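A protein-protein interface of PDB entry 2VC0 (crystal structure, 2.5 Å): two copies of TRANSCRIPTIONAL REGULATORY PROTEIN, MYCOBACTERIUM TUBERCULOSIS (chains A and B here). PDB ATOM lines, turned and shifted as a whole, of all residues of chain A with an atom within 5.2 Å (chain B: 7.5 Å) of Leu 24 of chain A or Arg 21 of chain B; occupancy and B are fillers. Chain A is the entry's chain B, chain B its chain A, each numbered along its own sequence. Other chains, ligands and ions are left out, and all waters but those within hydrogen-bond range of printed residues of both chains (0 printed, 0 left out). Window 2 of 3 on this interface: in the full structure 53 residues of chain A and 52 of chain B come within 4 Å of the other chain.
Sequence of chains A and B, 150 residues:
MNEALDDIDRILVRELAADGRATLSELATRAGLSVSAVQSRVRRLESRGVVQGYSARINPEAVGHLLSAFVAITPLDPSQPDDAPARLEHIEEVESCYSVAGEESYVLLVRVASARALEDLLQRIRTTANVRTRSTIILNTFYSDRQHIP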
ATOM      1  N   LEU A  16       0.589  -2.417 -18.960  1.00  0.00           N
ATOM      2  CA  LEU A  16       1.728  -2.591 -18.082  1.00  0.00           C
ATOM      3  C   LEU A  16       1.471  -2.290 -16.601  1.00  0.00           C
ATOM      4  O   LEU A  16       2.171  -2.817 -15.719  1.00  0.00           O
ATOM      5  CB  LEU A  16       2.946  -1.809 -18.594  1.00  0.00           C
ATOM      6  CG  LEU A  16       3.677  -2.578 -19.699  1.00  0.00           C
ATOM      7  CD1 LEU A  16       4.746  -1.696 -20.337  1.00  0.00           C
ATOM      8  CD2 LEU A  16       4.274  -3.903 -19.185  1.00  0.00           C
ATOM      9  N   GLY A  20       2.983  -6.154 -15.015  1.00  0.00           N
ATOM     10  CA  GLY A  20       4.355  -5.811 -15.347  1.00  0.00           C
ATOM     11  C   GLY A  20       5.099  -6.854 -16.176  1.00  0.00           C
ATOM     12  O   GLY A  20       6.143  -6.557 -16.756  1.00  0.00           O
ATOM     13  N   ARG A  21       4.559  -8.072 -16.231  1.00  0.00           N
ATOM     14  CA  ARG A  21       5.209  -9.165 -16.944  1.00  0.00           C
ATOM     15  C   ARG A  21       4.526  -9.524 -18.245  1.00  0.00           C
ATOM     16  O   ARG A  21       4.966 -10.458 -18.902  1.00  0.00           O
ATOM     17  CB  ARG A  21       5.324 -10.418 -16.074  1.00  0.00           C
ATOM     18  CG  ARG A  21       6.313 -10.284 -15.005  1.00  0.00           C
ATOM     19  CD  ARG A  21       6.354 -11.519 -14.171  1.00  0.00           C
ATOM     20  NE  ARG A  21       7.267 -12.543 -14.699  1.00  0.00           N
ATOM     21  CZ  ARG A  21       8.601 -12.518 -14.631  1.00  0.00           C
ATOM     22  NH1 ARG A  21       9.275 -11.513 -14.115  1.00  0.00           N
ATOM     23  NH2 ARG A  21       9.286 -13.519 -15.120  1.00  0.00           N
ATOM     24  N   ALA A  22       3.443  -8.836 -18.623  1.00  0.00           N
ATOM     25  CA  ALA A  22       2.985  -8.905 -20.014  1.00  0.00           C
ATOM     26  C   ALA A  22       4.260  -8.946 -20.855  1.00  0.00           C
ATOM     27  O   ALA A  22       5.262  -8.230 -20.564  1.00  0.00           O
ATOM     28  N   THR A  23       4.285  -9.820 -21.861  1.00  0.00           N
ATOM     29  CA  THR A  23       5.477  -9.854 -22.743  1.00  0.00           C
ATOM     30  C   THR A  23       5.291  -9.091 -24.026  1.00  0.00           C
ATOM     31  O   THR A  23       4.164  -9.026 -24.552  1.00  0.00           O
ATOM     32  CB  THR A  23       6.025 -11.280 -23.051  1.00  0.00           C
ATOM     33  OG1 THR A  23       5.024 -12.254 -22.712  1.00  0.00           O
ATOM     34  CG2 THR A  23       7.458 -11.569 -22.315  1.00  0.00           C
ATOM     35  N   LEU A  24       6.416  -8.525 -24.499  1.00  0.00           N
ATOM     36  CA  LEU A  24       6.517  -7.743 -25.749  1.00  0.00           C
ATOM     37  C   LEU A  24       5.572  -8.290 -26.837  1.00  0.00           C
ATOM     38  O   LEU A  24       4.870  -7.520 -27.506  1.00  0.00           O
ATOM     39  CB  LEU A  24       7.969  -7.750 -26.253  1.00  0.00           C
ATOM     40  CG  LEU A  24       9.027  -6.754 -25.751  1.00  0.00           C
ATOM     41  CD1 LEU A  24       8.665  -6.114 -24.393  1.00  0.00           C
ATOM     42  CD2 LEU A  24      10.456  -7.385 -25.714  1.00  0.00           C
ATOM     43  N   SER A  25       5.544  -9.621 -26.984  1.00  0.00           N
ATOM     44  CA  SER A  25       4.604 -10.278 -27.897  1.00  0.00           C
ATOM     45  C   SER A  25       3.094 -10.054 -27.598  1.00  0.00           C
ATOM     46  O   SER A  25       2.430  -9.412 -28.419  1.00  0.00           O
ATOM     47  CB  SER A  25       4.996 -11.758 -28.179  1.00  0.00           C
ATOM     48  OG  SER A  25       4.786 -12.658 -27.097  1.00  0.00           O
ATOM     49  N   GLU A  26       2.575 -10.533 -26.450  1.00  0.00           N
ATOM     50  CA  GLU A  26       1.124 -10.386 -26.074  1.00  0.00           C
ATOM     51  C   GLU A  26       0.654  -8.936 -25.971  1.00  0.00           C
ATOM     52  O   GLU A  26      -0.547  -8.664 -25.981  1.00  0.00           O
ATOM     53  CB  GLU A  26       0.759 -11.161 -24.778  1.00  0.00           C
ATOM     54  N   LEU A  27       1.600  -8.004 -25.891  1.00  0.00           N
ATOM     55  CA  LEU A  27       1.247  -6.593 -25.855  1.00  0.00           C
ATOM     56  C   LEU A  27       0.913  -6.209 -27.254  1.00  0.00           C
ATOM     57  O   LEU A  27      -0.274  -6.105 -27.568  1.00  0.00           O
ATOM     58  CB  LEU A  27       2.372  -5.705 -25.295  1.00  0.00           C
ATOM     59  CG  LEU A  27       2.518  -5.559 -23.770  1.00  0.00           C
ATOM     60  CD1 LEU A  27       3.643  -4.598 -23.470  1.00  0.00           C
ATOM     61  CD2 LEU A  27       1.230  -5.096 -23.129  1.00  0.00           C
ATOM     62  N   ALA A  28       1.951  -6.041 -28.086  1.00  0.00           N
ATOM     63  CA  ALA A  28       1.839  -5.826 -29.549  1.00  0.00           C
ATOM     64  C   ALA A  28       0.531  -6.266 -30.244  1.00  0.00           C
ATOM     65  O   ALA A  28       0.068  -5.562 -31.158  1.00  0.00           O
ATOM     66  CB  ALA A  28       3.050  -6.402 -30.270  1.00  0.00           C
ATOM     67  N   VAL A  35       6.092  -6.592 -32.586  1.00  0.00           N
ATOM     68  CA  VAL A  35       6.972  -6.855 -31.415  1.00  0.00           C
ATOM     69  C   VAL A  35       8.283  -6.034 -31.425  1.00  0.00           C
ATOM     70  O   VAL A  35       9.209  -6.279 -30.651  1.00  0.00           O
ATOM     71  CB  VAL A  35       7.213  -8.416 -31.115  1.00  0.00           C
ATOM     72  CG1 VAL A  35       5.884  -9.202 -31.106  1.00  0.00           C
ATOM     73  CG2 VAL A  35       8.241  -9.071 -32.081  1.00  0.00           C
ATOM     74  N   VAL A  38       6.116  -1.829 -30.704  1.00  0.00           N
ATOM     75  CA  VAL A  38       5.845  -2.011 -29.264  1.00  0.00           C
ATOM     76  C   VAL A  38       7.156  -1.957 -28.490  1.00  0.00           C
ATOM     77  O   VAL A  38       7.306  -1.174 -27.552  1.00  0.00           O
ATOM     78  CB  VAL A  38       5.086  -3.347 -28.949  1.00  0.00           C
ATOM     79  CG1 VAL A  38       5.500  -3.924 -27.622  1.00  0.00           C
ATOM     80  CG2 VAL A  38       3.616  -3.112 -28.948  1.00  0.00           C
ATOM     81  N   GLN A  39       8.125  -2.740 -28.935  1.00  0.00           N
ATOM     82  CA  GLN A  39       9.305  -2.912 -28.155  1.00  0.00           C
ATOM     83  C   GLN A  39      10.132  -1.656 -28.018  1.00  0.00           C
ATOM     84  O   GLN A  39      10.721  -1.410 -26.965  1.00  0.00           O
ATOM     85  CB  GLN A  39      10.154  -4.032 -28.720  1.00  0.00           C
ATOM     86  CG  GLN A  39      11.124  -4.574 -27.677  1.00  0.00           C
ATOM     87  CD  GLN A  39      12.432  -5.011 -28.271  1.00  0.00           C
ATOM     88  OE1 GLN A  39      13.497  -4.562 -27.839  1.00  0.00           O
ATOM     89  NE2 GLN A  39      12.365  -5.875 -29.287  1.00  0.00           N
ATOM     90  N   TYR A  54       9.750  -1.795 -12.664  1.00  0.00           N
ATOM     91  CA  TYR A  54       8.787  -2.866 -12.670  1.00  0.00           C
ATOM     92  C   TYR A  54       8.945  -3.510 -11.364  1.00  0.00           C
ATOM     93  O   TYR A  54      10.079  -3.659 -10.895  1.00  0.00           O
ATOM     94  CB  TYR A  54       9.092  -3.870 -13.770  1.00  0.00           C
ATOM     95  CG  TYR A  54       9.007  -3.223 -15.128  1.00  0.00           C
ATOM     96  CD1 TYR A  54      10.153  -2.581 -15.664  1.00  0.00           C
ATOM     97  CD2 TYR A  54       7.784  -3.173 -15.840  1.00  0.00           C
ATOM     98  CE1 TYR A  54      10.110  -1.935 -16.859  1.00  0.00           C
ATOM     99  CE2 TYR A  54       7.716  -2.537 -17.026  1.00  0.00           C
ATOM    100  CZ  TYR A  54       8.901  -1.909 -17.552  1.00  0.00           C
ATOM    101  OH  TYR A  54       8.920  -1.250 -18.782  1.00  0.00           O
ATOM    102  N   GLU B  15      14.634 -10.167  -5.407  1.00  0.00           N
ATOM    103  CA  GLU B  15      14.851  -9.898  -6.840  1.00  0.00           C
ATOM    104  C   GLU B  15      13.627  -9.451  -7.568  1.00  0.00           C
ATOM    105  O   GLU B  15      13.725  -8.580  -8.417  1.00  0.00           O
ATOM    106  CB  GLU B  15      15.388 -11.130  -7.578  1.00  0.00           C
ATOM    107  CG  GLU B  15      16.738 -11.611  -7.081  1.00  0.00           C
ATOM    108  CD  GLU B  15      17.774 -10.520  -7.079  1.00  0.00           C
ATOM    109  OE1 GLU B  15      17.805  -9.707  -8.053  1.00  0.00           O
ATOM    110  OE2 GLU B  15      18.547 -10.467  -6.093  1.00  0.00           O
ATOM    111  N   LEU B  16      12.470 -10.035  -7.316  1.00  0.00           N
ATOM    112  CA  LEU B  16      11.286  -9.578  -8.080  1.00  0.00           C
ATOM    113  C   LEU B  16      10.683  -8.231  -7.611  1.00  0.00           C
ATOM    114  O   LEU B  16       9.976  -7.558  -8.389  1.00  0.00           O
ATOM    115  CB  LEU B  16      10.187 -10.638  -8.155  1.00  0.00           C
ATOM    116  CG  LEU B  16      10.516 -11.917  -8.930  1.00  0.00           C
ATOM    117  CD1 LEU B  16       9.578 -13.030  -8.483  1.00  0.00           C
ATOM    118  CD2 LEU B  16      10.475 -11.752 -10.425  1.00  0.00           C
ATOM    119  N   ALA B  17      10.945  -7.864  -6.344  1.00  0.00           N
ATOM    120  CA  ALA B  17      10.594  -6.539  -5.817  1.00  0.00           C
ATOM    121  C   ALA B  17      11.445  -5.526  -6.553  1.00  0.00           C
ATOM    122  O   ALA B  17      10.907  -4.536  -7.033  1.00  0.00           O
ATOM    123  CB  ALA B  17      10.793  -6.456  -4.271  1.00  0.00           C
ATOM    124  N   ALA B  18      12.744  -5.807  -6.701  1.00  0.00           N
ATOM    125  CA  ALA B  18      13.652  -4.867  -7.395  1.00  0.00           C
ATOM    126  C   ALA B  18      13.393  -4.915  -8.908  1.00  0.00           C
ATOM    127  O   ALA B  18      13.329  -3.897  -9.563  1.00  0.00           O
ATOM    128  CB  ALA B  18      15.109  -5.116  -7.053  1.00  0.00           C
ATOM    129  N   ASP B  19      13.157  -6.099  -9.462  1.00  0.00           N
ATOM    130  CA  ASP B  19      12.911  -6.138 -10.888  1.00  0.00           C
ATOM    131  C   ASP B  19      11.834  -7.118 -11.271  1.00  0.00           C
ATOM    132  O   ASP B  19      12.087  -8.309 -11.307  1.00  0.00           O
ATOM    133  CB  ASP B  19      14.199  -6.491 -11.595  1.00  0.00           C
ATOM    134  CG  ASP B  19      14.032  -6.515 -13.115  1.00  0.00           C
ATOM    135  OD1 ASP B  19      12.979  -6.048 -13.689  1.00  0.00           O
ATOM    136  OD2 ASP B  19      15.010  -7.012 -13.733  1.00  0.00           O
ATOM    137  N   GLY B  20      10.644  -6.614 -11.566  1.00  0.00           N
ATOM    138  CA  GLY B  20       9.476  -7.477 -11.657  1.00  0.00           C
ATOM    139  C   GLY B  20       9.474  -8.161 -12.988  1.00  0.00           C
ATOM    140  O   GLY B  20       8.578  -8.920 -13.311  1.00  0.00           O
ATOM    141  N   ARG B  21      10.464  -7.831 -13.790  1.00  0.00           N
ATOM    142  CA  ARG B  21      10.620  -8.420 -15.115  1.00  0.00           C
ATOM    143  C   ARG B  21      11.921  -9.216 -15.263  1.00  0.00           C
ATOM    144  O   ARG B  21      12.225  -9.541 -16.375  1.00  0.00           O
ATOM    145  CB  ARG B  21      10.594  -7.339 -16.194  1.00  0.00           C
ATOM    146  CG  ARG B  21       9.258  -7.179 -16.849  1.00  0.00           C
ATOM    147  CD  ARG B  21       9.289  -5.983 -17.846  1.00  0.00           C
ATOM    148  NE  ARG B  21       9.363  -6.472 -19.226  1.00  0.00           N
ATOM    149  CZ  ARG B  21       8.307  -6.857 -19.944  1.00  0.00           C
ATOM    150  NH1 ARG B  21       7.065  -6.802 -19.438  1.00  0.00           N
ATOM    151  NH2 ARG B  21       8.500  -7.290 -21.192  1.00  0.00           N
ATOM    152  N   ALA B  22      12.694  -9.431 -14.172  1.00  0.00           N
ATOM    153  CA  ALA B  22      13.681 -10.497 -14.031  1.00  0.00           C
ATOM    154  C   ALA B  22      13.161 -11.647 -14.929  1.00  0.00           C
ATOM    155  O   ALA B  22      11.976 -12.069 -14.865  1.00  0.00           O
ATOM    156  N   THR B  23      13.991 -12.152 -15.833  1.00  0.00           N
ATOM    157  CA  THR B  23      13.538 -13.374 -16.454  1.00  0.00           C
ATOM    158  C   THR B  23      13.940 -14.608 -15.633  1.00  0.00           C
ATOM    159  O   THR B  23      14.877 -14.574 -14.810  1.00  0.00           O
ATOM    160  CB  THR B  23      14.048 -13.508 -17.887  1.00  0.00           C
ATOM    161  OG1 THR B  23      15.395 -13.008 -17.897  1.00  0.00           O
ATOM    162  CG2 THR B  23      13.124 -12.657 -18.917  1.00  0.00           C
ATOM    163  N   LEU B  24      13.215 -15.690 -15.885  1.00  0.00           N
ATOM    164  CA  LEU B  24      13.513 -16.956 -15.265  1.00  0.00           C
ATOM    165  C   LEU B  24      15.000 -17.323 -15.300  1.00  0.00           C
ATOM    166  O   LEU B  24      15.555 -17.571 -14.229  1.00  0.00           O
ATOM    167  CB  LEU B  24      12.658 -18.016 -15.899  1.00  0.00           C
ATOM    168  CG  LEU B  24      11.286 -18.267 -15.294  1.00  0.00           C
ATOM    169  CD1 LEU B  24      10.840 -17.290 -14.150  1.00  0.00           C
ATOM    170  CD2 LEU B  24      10.285 -18.374 -16.445  1.00  0.00           C
ATOM    171  N   GLU B  26      17.723 -15.412 -15.461  1.00  0.00           N
ATOM    172  CA  GLU B  26      18.378 -14.505 -14.472  1.00  0.00           C
ATOM    173  C   GLU B  26      18.130 -14.920 -13.019  1.00  0.00           C
ATOM    174  O   GLU B  26      19.090 -14.948 -12.199  1.00  0.00           O
ATOM    175  CB  GLU B  26      17.941 -13.061 -14.636  1.00  0.00           C
ATOM    176  CG  GLU B  26      18.314 -12.378 -16.007  1.00  0.00           C
ATOM    177  CD  GLU B  26      19.786 -11.838 -16.063  1.00  0.00           C
ATOM    178  OE1 GLU B  26      20.729 -12.560 -15.588  1.00  0.00           O
ATOM    179  OE2 GLU B  26      19.983 -10.678 -16.584  1.00  0.00           O
ATOM    180  N   LEU B  27      16.870 -15.233 -12.689  1.00  0.00           N
ATOM    181  CA  LEU B  27      16.524 -15.678 -11.329  1.00  0.00           C
ATOM    182  C   LEU B  27      17.193 -16.993 -10.945  1.00  0.00           C
ATOM    183  O   LEU B  27      17.844 -17.072  -9.910  1.00  0.00           O
ATOM    184  CB  LEU B  27      14.979 -15.739 -11.115  1.00  0.00           C
ATOM    185  CG  LEU B  27      14.234 -14.399 -11.407  1.00  0.00           C
ATOM    186  CD1 LEU B  27      12.722 -14.531 -11.353  1.00  0.00           C
ATOM    187  CD2 LEU B  27      14.720 -13.321 -10.483  1.00  0.00           C
ATOM    188  N   TYR B  54       2.183  -8.038 -10.616  1.00  0.00           N
ATOM    189  CA  TYR B  54       3.347  -7.339 -11.156  1.00  0.00           C
ATOM    190  C   TYR B  54       2.948  -6.054 -11.844  1.00  0.00           C
ATOM    191  O   TYR B  54       1.986  -6.062 -12.564  1.00  0.00           O
ATOM    192  CB  TYR B  54       3.986  -8.237 -12.212  1.00  0.00           C
ATOM    193  CG  TYR B  54       4.398  -9.553 -11.680  1.00  0.00           C
ATOM    194  CD1 TYR B  54       3.564 -10.642 -11.786  1.00  0.00           C
ATOM    195  CD2 TYR B  54       5.652  -9.700 -11.069  1.00  0.00           C
ATOM    196  CE1 TYR B  54       3.946 -11.901 -11.266  1.00  0.00           C
ATOM    197  CE2 TYR B  54       6.075 -10.921 -10.538  1.00  0.00           C
ATOM    198  CZ  TYR B  54       5.201 -12.031 -10.657  1.00  0.00           C
ATOM    199  OH  TYR B  54       5.603 -13.251 -10.148  1.00  0.00           O
ATOM    200  N   SER B  55       3.696  -4.976 -11.702  1.00  0.00           N
ATOM    201  CA  SER B  55       3.188  -3.695 -12.174  1.00  0.00           C
ATOM    202  C   SER B  55       4.311  -2.842 -12.614  1.00  0.00           C
ATOM    203  O   SER B  55       5.401  -2.823 -11.985  1.00  0.00           O
ATOM    204  CB  SER B  55       2.404  -2.929 -11.035  1.00  0.00           C
ATOM    205  N   ALA B  56       4.073  -2.109 -13.694  1.00  0.00           N
ATOM    206  CA  ALA B  56       4.976  -0.999 -14.043  1.00  0.00           C
ATOM    207  C   ALA B  56       4.698   0.133 -13.040  1.00  0.00           C
ATOM    208  O   ALA B  56       3.543   0.437 -12.768  1.00  0.00           O
ATOM    209  CB  ALA B  56       4.744  -0.547 -15.476  1.00  0.00           C
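The backbone carbonyl oxygen (O) of Tyr 54 of chain B lies within hydrogen-bond range of the backbone NH (N) of Gly 20 of chain A (2.6 Å). O of Gly 20 of chain B lies within hydrogen-bond range of NH1 of Arg 21 of chain A. The backbone NH (N) of Ala 56 of chain B is in hydrogen-bond range of the backbone carbonyl oxygen (O) of Leu 16 of chain A (2.9 Å). NH1 of Arg 21 of chain B is in hydrogen-bond range of O of Gly 20 of chain A (2.8 Å). The guanidinium group (NH1) of Arg 21 of chain B sits at hydrogen-bond distance from the backbone carbonyl oxygen (O) of Ala 22 of chain A (2.6 Å). The backbone NH (N) of Gly 20 of chain B is in hydrogen-bond range of the backbone carbonyl oxygen (O) of Tyr 54 of chain A. O of Ala 22 of chain B sits at hydrogen-bond distance from NH1 of Arg 21 of chain A.
The side-chain carboxylate (OD1) of Asp 19 of chain B lies close to the backbone NH (N) of Arg 21 of chain B (3.1 Å). The side-chain carboxylate of Asp 19 of chain B sits at hydrogen-bond distance from the backbone NH of Ala 22 of chain B, at 3.4 Å.
Among the printed residues, pairs that only touch across the chains: Leu 24 of chain A with Arg 21 of chain B (3.4 Å), Tyr 54 of chain A with Ser 55 of chain B (3.5 Å), Arg 21 of chain A with Arg 21 of chain B (3.5 Å), Tyr 54 of chain A with Ala 18 of chain B (3.5 Å), Gly 20 of chain A with Ser 55 of chain B (3.6 Å), Arg 21 of chain A with Tyr 54 of chain B (3.7 Å), Tyr 54 of chain A with Asp 19 of chain B (3.8 Å), Tyr 54 of chain A with Arg 21 of chain B (3.8 Å), Leu 16 of chain A with Ser 55 of chain B (3.8 Å), Arg 21 of chain A with Leu 16 of chain B (3.9 Å) and Tyr 54 of chain A with Ala 56 of chain B (3.9 Å).
Of the printed residues of chain B, Arg 21 of chain A touches Leu 16, Gly 20, Arg 21, Ala 22 and Tyr 54. Of chain B, only Arg 21 (3.4 Å) comes within 4 Å of Leu 24 of chain A. Of the printed residues of chain B, Tyr 54 of chain A touches Ala 18, Asp 19, Gly 20, Arg 21, Ser 55 and Ala 56. Arg 21 of chain B touches just these residues of chain A: Gly 20, Arg 21, Ala 22, Leu 24 and Tyr 54. Of the printed residues of chain A, Ser 55 of chain B touches Leu 16 (3.8 Å), Gly 20 (3.6 Å) and Tyr 54 (3.5 Å). The nearest printed residue of chain B that does not touch Leu 24 of chain A is Thr 23 of chain B (9.0 Å). The nearest residue of chain A that does not touch Arg 21 of chain B is Leu 16 of chain A (4.03 Å). The nearest printed residue of chain A that does not touch Ala 56 of chain B is Gly 20 of chain A (4.1 Å).
Of the 15 printed residues of chain B, 9 touch a printed residue of chain A. Printed residues of chain A that touch a printed residue of chain B: Leu 16, Gly 20, Arg 21, Ala 22, Leu 24 and Tyr 54.
Gly 20 of chain A touches Arg 21 of chain B, and with the chains exchanged Arg 21 of chain A touches Gly 20 of chain B. Gly 20 of chain A touches Tyr 54 of chain B, and with the chains exchanged Tyr 54 of chain A touches Gly 20 of chain B. Arg 21 of chain A touches Tyr 54 of chain B, and with the chains exchanged Tyr 54 of chain A touches Arg 21 of chain B. Leu 24 of chain A touches Arg 21 of chain B, but with the chains exchanged Arg 21 of chain A does not touch Leu 24 of chain B (4.2 Å).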
